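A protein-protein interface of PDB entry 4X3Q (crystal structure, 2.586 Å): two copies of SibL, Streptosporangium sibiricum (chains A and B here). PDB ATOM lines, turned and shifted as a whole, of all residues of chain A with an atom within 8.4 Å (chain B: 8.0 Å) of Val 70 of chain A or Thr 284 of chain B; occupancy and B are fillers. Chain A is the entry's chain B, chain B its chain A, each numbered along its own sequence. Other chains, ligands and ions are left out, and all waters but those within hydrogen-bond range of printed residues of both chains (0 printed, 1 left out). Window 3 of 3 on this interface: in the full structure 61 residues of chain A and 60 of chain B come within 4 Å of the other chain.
No position is printed for both chains.
Hydrophobic or aromatic side chains of chain A within 4 Å of the printed part of chain B: Leu 60, Ala 64, Leu 65 and Val 70.
Of the 12 printed residues of chain B, 6 touch a printed residue of chain A.
OD1 of Asp 282 of chain B is in hydrogen-bond range of OG1 of Thr 284 of chain B (2.8 Å).
The backbone NH of Asp 280 of chain B lies within hydrogen-bond range of the backbone carbonyl oxygen of Gly 285 of chain B.
Leu 60 of chain A touches Thr 279 of chain B (CD2 to OG1, 3.5 Å).
O of Arg 283 of chain B touches CD1 of Leu 60 of chain A, at 3.1 Å.
Thr 284 of chain B touches Leu 60 of chain A.
Leu 60 of chain A touches Gly 285 of chain B.
O of Leu 60 of chain A touches CB of Ala 290 of chain B, 3.7 Å away.
Ala 64 of chain A touches Thr 284 of chain B.
Ala 64 of chain A touches Ala 290 of chain B (CB to CB, 3.5 Å).
CD2 of Leu 65 of chain A touches CD1 of Leu 287 of chain B, at 3.8 Å.
Val 70 of chain A touches Thr 284 of chain B.
Of the printed residues of chain B, Leu 60 of chain A touches Thr 279, Arg 283, Thr 284, Gly 285 and Ala 290.
Val 70 of chain A touches one residue of chain B.
Of the printed residues of chain A, Arg 283 of chain B touches Leu 60 (3.1 Å).
Printed residues of chain A within 4 Å of Thr 284 of chain B: Leu 60, Ala 64 and Val 70.
Of the printed residues of chain A, Leu 287 of chain B touches Leu 65.
The nearest printed residue of chain B that does not touch Val 70 of chain A is Arg 283 of chain B (4.9 Å).
The nearest residue of chain A that does not touch Thr 284 of chain B is Thr 63 of chain A (4.4 Å).
The nearest printed residue of chain B that does not touch Leu 60 of chain A is Ala 289 of chain B (4.6 Å).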
ATOM      1  N   LEU A  33     -37.054  27.548  24.965  1.00  0.00           N
ATOM      2  CA  LEU A  33     -36.172  26.839  25.871  1.00  0.00           C
ATOM      3  C   LEU A  33     -36.556  27.141  27.314  1.00  0.00           C
ATOM      4  O   LEU A  33     -36.406  26.298  28.195  1.00  0.00           O
ATOM      5  CB  LEU A  33     -34.694  27.198  25.606  1.00  0.00           C
ATOM      6  CG  LEU A  33     -34.087  26.735  24.264  1.00  0.00           C
ATOM      7  CD1 LEU A  33     -32.577  26.915  24.248  1.00  0.00           C
ATOM      8  CD2 LEU A  33     -34.468  25.309  23.947  1.00  0.00           C
ATOM      9  N   PRO A  38     -35.028  21.146  28.963  1.00  0.00           N
ATOM     10  CA  PRO A  38     -34.078  20.965  27.860  1.00  0.00           C
ATOM     11  C   PRO A  38     -34.736  20.293  26.667  1.00  0.00           C
ATOM     12  O   PRO A  38     -35.693  19.531  26.861  1.00  0.00           O
ATOM     13  CB  PRO A  38     -33.004  20.068  28.471  1.00  0.00           C
ATOM     14  CG  PRO A  38     -33.757  19.244  29.451  1.00  0.00           C
ATOM     15  CD  PRO A  38     -34.864  20.108  29.994  1.00  0.00           C
ATOM     16  N   LEU A  39     -34.241  20.581  25.461  1.00  0.00           N
ATOM     17  CA  LEU A  39     -34.816  20.024  24.234  1.00  0.00           C
ATOM     18  C   LEU A  39     -33.765  19.503  23.257  1.00  0.00           C
ATOM     19  O   LEU A  39     -32.634  20.002  23.209  1.00  0.00           O
ATOM     20  CB  LEU A  39     -35.682  21.065  23.534  1.00  0.00           C
ATOM     21  CG  LEU A  39     -37.000  21.426  24.197  1.00  0.00           C
ATOM     22  CD1 LEU A  39     -37.711  22.483  23.371  1.00  0.00           C
ATOM     23  CD2 LEU A  39     -37.865  20.205  24.369  1.00  0.00           C
ATOM     24  N   SER A  40     -34.137  18.485  22.490  1.00  0.00           N
ATOM     25  CA  SER A  40     -33.268  18.013  21.424  1.00  0.00           C
ATOM     26  C   SER A  40     -33.320  19.004  20.291  1.00  0.00           C
ATOM     27  O   SER A  40     -34.272  19.788  20.179  1.00  0.00           O
ATOM     28  CB  SER A  40     -33.684  16.638  20.902  1.00  0.00           C
ATOM     29  OG  SER A  40     -34.837  16.722  20.083  1.00  0.00           O
ATOM     30  N   ALA A  41     -32.289  18.956  19.455  1.00  0.00           N
ATOM     31  CA  ALA A  41     -32.225  19.782  18.270  1.00  0.00           C
ATOM     32  C   ALA A  41     -33.460  19.563  17.413  1.00  0.00           C
ATOM     33  O   ALA A  41     -34.055  20.514  16.915  1.00  0.00           O
ATOM     34  CB  ALA A  41     -30.979  19.467  17.481  1.00  0.00           C
ATOM     35  N   LEU A  59     -28.603  26.597  16.654  1.00  0.00           N
ATOM     36  CA  LEU A  59     -28.181  26.057  17.949  1.00  0.00           C
ATOM     37  C   LEU A  59     -26.673  26.076  18.134  1.00  0.00           C
ATOM     38  O   LEU A  59     -26.193  26.266  19.243  1.00  0.00           O
ATOM     39  CB  LEU A  59     -28.693  24.633  18.132  1.00  0.00           C
ATOM     40  CG  LEU A  59     -30.188  24.578  18.430  1.00  0.00           C
ATOM     41  CD1 LEU A  59     -30.682  23.151  18.418  1.00  0.00           C
ATOM     42  CD2 LEU A  59     -30.458  25.240  19.765  1.00  0.00           C
ATOM     43  N   LEU A  60     -25.921  25.904  17.052  1.00  0.00           N
ATOM     44  CA  LEU A  60     -24.461  25.980  17.136  1.00  0.00           C
ATOM     45  C   LEU A  60     -24.034  27.411  17.468  1.00  0.00           C
ATOM     46  O   LEU A  60     -23.153  27.644  18.296  1.00  0.00           O
ATOM     47  CB  LEU A  60     -23.818  25.511  15.824  1.00  0.00           C
ATOM     48  CG  LEU A  60     -22.290  25.554  15.796  1.00  0.00           C
ATOM     49  CD1 LEU A  60     -21.767  24.613  16.878  1.00  0.00           C
ATOM     50  CD2 LEU A  60     -21.737  25.189  14.424  1.00  0.00           C
ATOM     51  N   GLY A  61     -24.684  28.374  16.823  1.00  0.00           N
ATOM     52  CA  GLY A  61     -24.396  29.771  17.058  1.00  0.00           C
ATOM     53  C   GLY A  61     -24.680  30.182  18.494  1.00  0.00           C
ATOM     54  O   GLY A  61     -23.833  30.786  19.135  1.00  0.00           O
ATOM     55  N   THR A  62     -25.863  29.850  19.001  1.00  0.00           N
ATOM     56  CA  THR A  62     -26.252  30.294  20.333  1.00  0.00           C
ATOM     57  C   THR A  62     -25.466  29.561  21.397  1.00  0.00           C
ATOM     58  O   THR A  62     -25.100  30.154  22.421  1.00  0.00           O
ATOM     59  CB  THR A  62     -27.760  30.098  20.603  1.00  0.00           C
ATOM     60  OG1 THR A  62     -28.108  28.719  20.429  1.00  0.00           O
ATOM     61  CG2 THR A  62     -28.589  30.986  19.667  1.00  0.00           C
ATOM     62  N   THR A  63     -25.193  28.278  21.150  1.00  0.00           N
ATOM     63  CA  THR A  63     -24.405  27.492  22.094  1.00  0.00           C
ATOM     64  C   THR A  63     -22.986  28.022  22.149  1.00  0.00           C
ATOM     65  O   THR A  63     -22.449  28.244  23.228  1.00  0.00           O
ATOM     66  CB  THR A  63     -24.344  26.004  21.730  1.00  0.00           C
ATOM     67  OG1 THR A  63     -25.668  25.468  21.646  1.00  0.00           O
ATOM     68  CG2 THR A  63     -23.576  25.244  22.794  1.00  0.00           C
ATOM     69  N   ALA A  64     -22.381  28.261  20.991  1.00  0.00           N
ATOM     70  CA  ALA A  64     -20.999  28.728  20.981  1.00  0.00           C
ATOM     71  C   ALA A  64     -20.887  30.095  21.622  1.00  0.00           C
ATOM     72  O   ALA A  64     -19.836  30.471  22.126  1.00  0.00           O
ATOM     73  CB  ALA A  64     -20.453  28.762  19.564  1.00  0.00           C
ATOM     74  N   LEU A  65     -21.974  30.847  21.581  1.00  0.00           N
ATOM     75  CA  LEU A  65     -21.971  32.192  22.129  1.00  0.00           C
ATOM     76  C   LEU A  65     -22.319  32.201  23.619  1.00  0.00           C
ATOM     77  O   LEU A  65     -22.157  33.213  24.292  1.00  0.00           O
ATOM     78  CB  LEU A  65     -22.929  33.085  21.343  1.00  0.00           C
ATOM     79  CG  LEU A  65     -22.366  33.614  20.015  1.00  0.00           C
ATOM     80  CD1 LEU A  65     -23.474  34.312  19.255  1.00  0.00           C
ATOM     81  CD2 LEU A  65     -21.151  34.560  20.192  1.00  0.00           C
ATOM     82  N   GLY A  66     -22.769  31.063  24.131  1.00  0.00           N
ATOM     83  CA  GLY A  66     -23.211  30.985  25.505  1.00  0.00           C
ATOM     84  C   GLY A  66     -24.647  31.426  25.699  1.00  0.00           C
ATOM     85  O   GLY A  66     -25.136  31.439  26.825  1.00  0.00           O
ATOM     86  N   LEU A  67     -25.330  31.818  24.625  1.00  0.00           N
ATOM     87  CA  LEU A  67     -26.744  32.185  24.755  1.00  0.00           C
ATOM     88  C   LEU A  67     -27.563  30.964  25.098  1.00  0.00           C
ATOM     89  O   LEU A  67     -28.634  31.073  25.687  1.00  0.00           O
ATOM     90  CB  LEU A  67     -27.294  32.820  23.486  1.00  0.00           C
ATOM     91  CG  LEU A  67     -26.494  34.009  22.984  1.00  0.00           C
ATOM     92  CD1 LEU A  67     -27.255  34.600  21.818  1.00  0.00           C
ATOM     93  CD2 LEU A  67     -26.220  35.032  24.086  1.00  0.00           C
ATOM     94  N   SER A  68     -27.056  29.805  24.700  1.00  0.00           N
ATOM     95  CA  SER A  68     -27.616  28.532  25.120  1.00  0.00           C
ATOM     96  C   SER A  68     -26.488  27.611  25.571  1.00  0.00           C
ATOM     97  O   SER A  68     -25.318  27.918  25.373  1.00  0.00           O
ATOM     98  CB  SER A  68     -28.425  27.893  23.989  1.00  0.00           C
ATOM     99  OG  SER A  68     -27.606  27.611  22.871  1.00  0.00           O
ATOM    100  N   THR A  69     -26.833  26.513  26.227  1.00  0.00           N
ATOM    101  CA  THR A  69     -25.828  25.524  26.594  1.00  0.00           C
ATOM    102  C   THR A  69     -26.332  24.162  26.186  1.00  0.00           C
ATOM    103  O   THR A  69     -27.549  23.927  26.107  1.00  0.00           O
ATOM    104  CB  THR A  69     -25.515  25.470  28.103  1.00  0.00           C
ATOM    105  OG1 THR A  69     -26.683  25.049  28.812  1.00  0.00           O
ATOM    106  CG2 THR A  69     -25.011  26.818  28.620  1.00  0.00           C
ATOM    107  N   VAL A  70     -25.399  23.260  25.916  1.00  0.00           N
ATOM    108  CA  VAL A  70     -25.789  21.907  25.574  1.00  0.00           C
ATOM    109  C   VAL A  70     -25.036  20.929  26.463  1.00  0.00           C
ATOM    110  O   VAL A  70     -23.811  20.854  26.478  1.00  0.00           O
ATOM    111  CB  VAL A  70     -25.553  21.597  24.057  1.00  0.00           C
ATOM    112  CG1 VAL A  70     -24.113  21.836  23.649  1.00  0.00           C
ATOM    113  CG2 VAL A  70     -26.022  20.196  23.707  1.00  0.00           C
ATOM    114  N   THR A  71     -25.824  20.166  27.196  1.00  0.00           N
ATOM    115  CA  THR A  71     -25.368  19.052  27.992  1.00  0.00           C
ATOM    116  C   THR A  71     -26.323  18.028  27.501  1.00  0.00           C
ATOM    117  O   THR A  71     -27.046  18.335  26.566  1.00  0.00           O
ATOM    118  CB  THR A  71     -25.578  19.267  29.476  1.00  0.00           C
ATOM    119  OG1 THR A  71     -26.978  19.149  29.757  1.00  0.00           O
ATOM    120  CG2 THR A  71     -25.076  20.649  29.899  1.00  0.00           C
ATOM    121  N   ASP A  72     -26.322  16.809  28.027  1.00  0.00           N
ATOM    122  CA  ASP A  72     -27.468  15.956  27.739  1.00  0.00           C
ATOM    123  C   ASP A  72     -27.634  15.603  26.245  1.00  0.00           C
ATOM    124  O   ASP A  72     -28.150  14.540  25.896  1.00  0.00           O
ATOM    125  CB  ASP A  72     -28.699  16.732  28.313  1.00  0.00           C
ATOM    126  CG  ASP A  72     -30.053  16.071  28.085  1.00  0.00           C
ATOM    127  OD1 ASP A  72     -30.203  15.142  27.268  1.00  0.00           O
ATOM    128  OD2 ASP A  72     -31.014  16.531  28.747  1.00  0.00           O
ATOM    129  N   GLY A  73     -27.108  16.462  25.374  1.00  0.00           N
ATOM    130  CA  GLY A  73     -27.485  16.503  23.968  1.00  0.00           C
ATOM    131  C   GLY A  73     -28.852  17.188  23.919  1.00  0.00           C
ATOM    132  O   GLY A  73     -29.542  17.193  22.891  1.00  0.00           O
ATOM    133  N   GLY A  74     -29.212  17.787  25.058  1.00  0.00           N
ATOM    134  CA  GLY A  74     -30.408  18.590  25.250  1.00  0.00           C
ATOM    135  C   GLY A  74     -30.018  20.043  25.432  1.00  0.00           C
ATOM    136  O   GLY A  74     -28.968  20.362  26.014  1.00  0.00           O
ATOM    137  N   TYR A  75     -30.840  20.943  24.916  1.00  0.00           N
ATOM    138  CA  TYR A  75     -30.468  22.355  24.941  1.00  0.00           C
ATOM    139  C   TYR A  75     -31.267  23.192  25.943  1.00  0.00           C
ATOM    140  O   TYR A  75     -32.493  23.048  26.067  1.00  0.00           O
ATOM    141  CB  TYR A  75     -30.636  22.946  23.544  1.00  0.00           C
ATOM    142  CG  TYR A  75     -29.629  22.473  22.531  1.00  0.00           C
ATOM    143  CD1 TYR A  75     -29.875  21.345  21.760  1.00  0.00           C
ATOM    144  CD2 TYR A  75     -28.427  23.154  22.353  1.00  0.00           C
ATOM    145  CE1 TYR A  75     -28.969  20.912  20.837  1.00  0.00           C
ATOM    146  CE2 TYR A  75     -27.506  22.732  21.427  1.00  0.00           C
ATOM    147  CZ  TYR A  75     -27.782  21.609  20.672  1.00  0.00           C
ATOM    148  OH  TYR A  75     -26.859  21.195  19.750  1.00  0.00           O
ATOM    149  N   ARG A  76     -30.548  24.086  26.622  1.00  0.00           N
ATOM    150  CA  ARG A  76     -31.127  25.043  27.555  1.00  0.00           C
ATOM    151  C   ARG A  76     -30.582  26.453  27.359  1.00  0.00           C
ATOM    152  O   ARG A  76     -29.557  26.653  26.699  1.00  0.00           O
ATOM    153  CB  ARG A  76     -30.896  24.597  29.003  1.00  0.00           C
ATOM    154  CG  ARG A  76     -31.883  23.543  29.486  1.00  0.00           C
ATOM    155  CD  ARG A  76     -33.177  24.249  29.986  1.00  0.00           C
ATOM    156  NE  ARG A  76     -33.809  23.586  31.136  1.00  0.00           N
ATOM    157  CZ  ARG A  76     -33.835  24.090  32.369  1.00  0.00           C
ATOM    158  NH1 ARG A  76     -33.257  25.260  32.623  1.00  0.00           N
ATOM    159  NH2 ARG A  76     -34.427  23.418  33.353  1.00  0.00           N
ATOM    160  N   ASN A  77     -31.282  27.426  27.939  1.00  0.00           N
ATOM    161  CA  ASN A  77     -30.816  28.790  27.882  1.00  0.00           C
ATOM    162  C   ASN A  77     -29.535  28.893  28.676  1.00  0.00           C
ATOM    163  O   ASN A  77     -29.384  28.261  29.727  1.00  0.00           O
ATOM    164  CB  ASN A  77     -31.871  29.756  28.414  1.00  0.00           C
ATOM    165  CG  ASN A  77     -33.035  29.914  27.461  1.00  0.00           C
ATOM    166  OD1 ASN A  77     -32.882  29.707  26.256  1.00  0.00           O
ATOM    167  ND2 ASN A  77     -34.197  30.318  27.980  1.00  0.00           N
ATOM    168  N   GLY A  78     -28.596  29.664  28.144  1.00  0.00           N
ATOM    169  CA  GLY A  78     -27.347  29.941  28.825  1.00  0.00           C
ATOM    170  C   GLY A  78     -27.602  30.985  29.884  1.00  0.00           C
ATOM    171  O   GLY A  78     -28.700  31.549  29.954  1.00  0.00           O
ATOM    172  N   THR B 279     -16.992  22.023  11.796  1.00  0.00           N
ATOM    173  CA  THR B 279     -17.663  22.109  13.084  1.00  0.00           C
ATOM    174  C   THR B 279     -17.240  20.932  13.943  1.00  0.00           C
ATOM    175  O   THR B 279     -17.257  19.787  13.482  1.00  0.00           O
ATOM    176  CB  THR B 279     -19.190  22.116  12.936  1.00  0.00           C
ATOM    177  OG1 THR B 279     -19.590  23.335  12.292  1.00  0.00           O
ATOM    178  CG2 THR B 279     -19.868  22.009  14.315  1.00  0.00           C
ATOM    179  N   ASP B 280     -16.881  21.209  15.194  1.00  0.00           N
ATOM    180  CA  ASP B 280     -16.546  20.146  16.129  1.00  0.00           C
ATOM    181  C   ASP B 280     -17.681  19.136  16.192  1.00  0.00           C
ATOM    182  O   ASP B 280     -18.857  19.497  16.060  1.00  0.00           O
ATOM    183  CB  ASP B 280     -16.251  20.720  17.507  1.00  0.00           C
ATOM    184  CG  ASP B 280     -15.063  21.649  17.495  1.00  0.00           C
ATOM    185  OD1 ASP B 280     -14.345  21.689  16.476  1.00  0.00           O
ATOM    186  OD2 ASP B 280     -14.841  22.351  18.496  1.00  0.00           O
ATOM    187  N   ASP B 281     -17.321  17.865  16.356  1.00  0.00           N
ATOM    188  CA  ASP B 281     -18.300  16.782  16.315  1.00  0.00           C
ATOM    189  C   ASP B 281     -19.311  16.898  17.450  1.00  0.00           C
ATOM    190  O   ASP B 281     -20.421  16.374  17.334  1.00  0.00           O
ATOM    191  CB  ASP B 281     -17.599  15.415  16.369  1.00  0.00           C
ATOM    192  CG  ASP B 281     -16.834  15.081  15.077  1.00  0.00           C
ATOM    193  OD1 ASP B 281     -17.279  15.487  13.975  1.00  0.00           O
ATOM    194  OD2 ASP B 281     -15.759  14.437  15.169  1.00  0.00           O
ATOM    195  N   ASP B 282     -18.928  17.559  18.548  1.00  0.00           N
ATOM    196  CA  ASP B 282     -19.838  17.701  19.688  1.00  0.00           C
ATOM    197  C   ASP B 282     -20.801  18.877  19.520  1.00  0.00           C
ATOM    198  O   ASP B 282     -21.584  19.159  20.414  1.00  0.00           O
ATOM    199  CB  ASP B 282     -19.044  17.834  21.009  1.00  0.00           C
ATOM    200  CG  ASP B 282     -18.259  19.143  21.136  1.00  0.00           C
ATOM    201  OD1 ASP B 282     -18.499  20.113  20.384  1.00  0.00           O
ATOM    202  OD2 ASP B 282     -17.343  19.186  21.991  1.00  0.00           O
ATOM    203  N   ARG B 283     -20.691  19.580  18.392  1.00  0.00           N
ATOM    204  CA  ARG B 283     -21.602  20.664  18.002  1.00  0.00           C
ATOM    205  C   ARG B 283     -21.607  21.874  18.931  1.00  0.00           C
ATOM    206  O   ARG B 283     -22.622  22.541  19.056  1.00  0.00           O
ATOM    207  CB  ARG B 283     -23.031  20.132  17.869  1.00  0.00           C
ATOM    208  CG  ARG B 283     -23.195  19.156  16.728  1.00  0.00           C
ATOM    209  CD  ARG B 283     -24.596  18.644  16.622  1.00  0.00           C
ATOM    210  NE  ARG B 283     -24.777  17.901  15.381  1.00  0.00           N
ATOM    211  CZ  ARG B 283     -24.615  16.589  15.279  1.00  0.00           C
ATOM    212  NH1 ARG B 283     -24.263  15.884  16.347  1.00  0.00           N
ATOM    213  NH2 ARG B 283     -24.798  15.986  14.113  1.00  0.00           N
ATOM    214  N   THR B 284     -20.473  22.173  19.559  1.00  0.00           N
ATOM    215  CA  THR B 284     -20.397  23.294  20.499  1.00  0.00           C
ATOM    216  C   THR B 284     -19.491  24.393  19.979  1.00  0.00           C
ATOM    217  O   THR B 284     -19.309  25.412  20.630  1.00  0.00           O
ATOM    218  CB  THR B 284     -19.909  22.863  21.899  1.00  0.00           C
ATOM    219  OG1 THR B 284     -18.531  22.471  21.843  1.00  0.00           O
ATOM    220  CG2 THR B 284     -20.762  21.712  22.424  1.00  0.00           C
ATOM    221  N   GLY B 285     -18.876  24.166  18.827  1.00  0.00           N
ATOM    222  CA  GLY B 285     -17.965  25.152  18.295  1.00  0.00           C
ATOM    223  C   GLY B 285     -17.190  24.646  17.101  1.00  0.00           C
ATOM    224  O   GLY B 285     -17.576  23.669  16.458  1.00  0.00           O
ATOM    225  N   PRO B 286     -16.084  25.317  16.784  1.00  0.00           N
ATOM    226  CA  PRO B 286     -15.602  26.521  17.468  1.00  0.00           C
ATOM    227  C   PRO B 286     -16.433  27.753  17.142  1.00  0.00           C
ATOM    228  O   PRO B 286     -17.319  27.704  16.290  1.00  0.00           O
ATOM    229  CB  PRO B 286     -14.174  26.689  16.945  1.00  0.00           C
ATOM    230  CG  PRO B 286     -14.090  25.881  15.761  1.00  0.00           C
ATOM    231  CD  PRO B 286     -15.184  24.881  15.711  1.00  0.00           C
ATOM    232  N   LEU B 287     -16.138  28.847  17.826  1.00  0.00           N
ATOM    233  CA  LEU B 287     -16.846  30.096  17.608  1.00  0.00           C
ATOM    234  C   LEU B 287     -16.849  30.513  16.121  1.00  0.00           C
ATOM    235  O   LEU B 287     -17.902  30.906  15.582  1.00  0.00           O
ATOM    236  CB  LEU B 287     -16.206  31.191  18.456  1.00  0.00           C
ATOM    237  CG  LEU B 287     -16.852  32.561  18.404  1.00  0.00           C
ATOM    238  CD1 LEU B 287     -18.258  32.442  18.991  1.00  0.00           C
ATOM    239  CD2 LEU B 287     -16.004  33.546  19.205  1.00  0.00           C
ATOM    240  N   ALA B 289     -16.689  28.729  13.314  1.00  0.00           N
ATOM    241  CA  ALA B 289     -17.650  28.013  12.483  1.00  0.00           C
ATOM    242  C   ALA B 289     -19.040  28.501  12.832  1.00  0.00           C
ATOM    243  O   ALA B 289     -19.890  28.744  11.961  1.00  0.00           O
ATOM    244  CB  ALA B 289     -17.552  26.497  12.691  1.00  0.00           C
ATOM    245  N   ALA B 290     -19.260  28.649  14.131  1.00  0.00           N
ATOM    246  CA  ALA B 290     -20.559  29.027  14.620  1.00  0.00           C
ATOM    247  C   ALA B 290     -20.968  30.364  14.020  1.00  0.00           C
ATOM    248  O   ALA B 290     -22.118  30.526  13.565  1.00  0.00           O
ATOM    249  CB  ALA B 290     -20.540  29.107  16.121  1.00  0.00           C
ATOM    250  N   ARG B 308     -19.622  18.941  10.285  1.00  0.00           N
ATOM    251  CA  ARG B 308     -18.769  18.323  11.290  1.00  0.00           C
ATOM    252  C   ARG B 308     -17.769  17.395  10.605  1.00  0.00           C
ATOM    253  O   ARG B 308     -18.102  16.774   9.583  1.00  0.00           O
ATOM    254  CB  ARG B 308     -19.591  17.518  12.303  1.00  0.00           C
ATOM    255  CG  ARG B 308     -20.607  18.329  13.036  1.00  0.00           C
ATOM    256  CD  ARG B 308     -21.792  17.489  13.445  1.00  0.00           C
ATOM    257  NE  ARG B 308     -21.461  16.556  14.512  1.00  0.00           N
ATOM    258  CZ  ARG B 308     -21.666  15.241  14.479  1.00  0.00           C
ATOM    259  NH1 ARG B 308     -22.182  14.657  13.400  1.00  0.00           N
ATOM    260  NH2 ARG B 308     -21.332  14.511  15.536  1.00  0.00           N
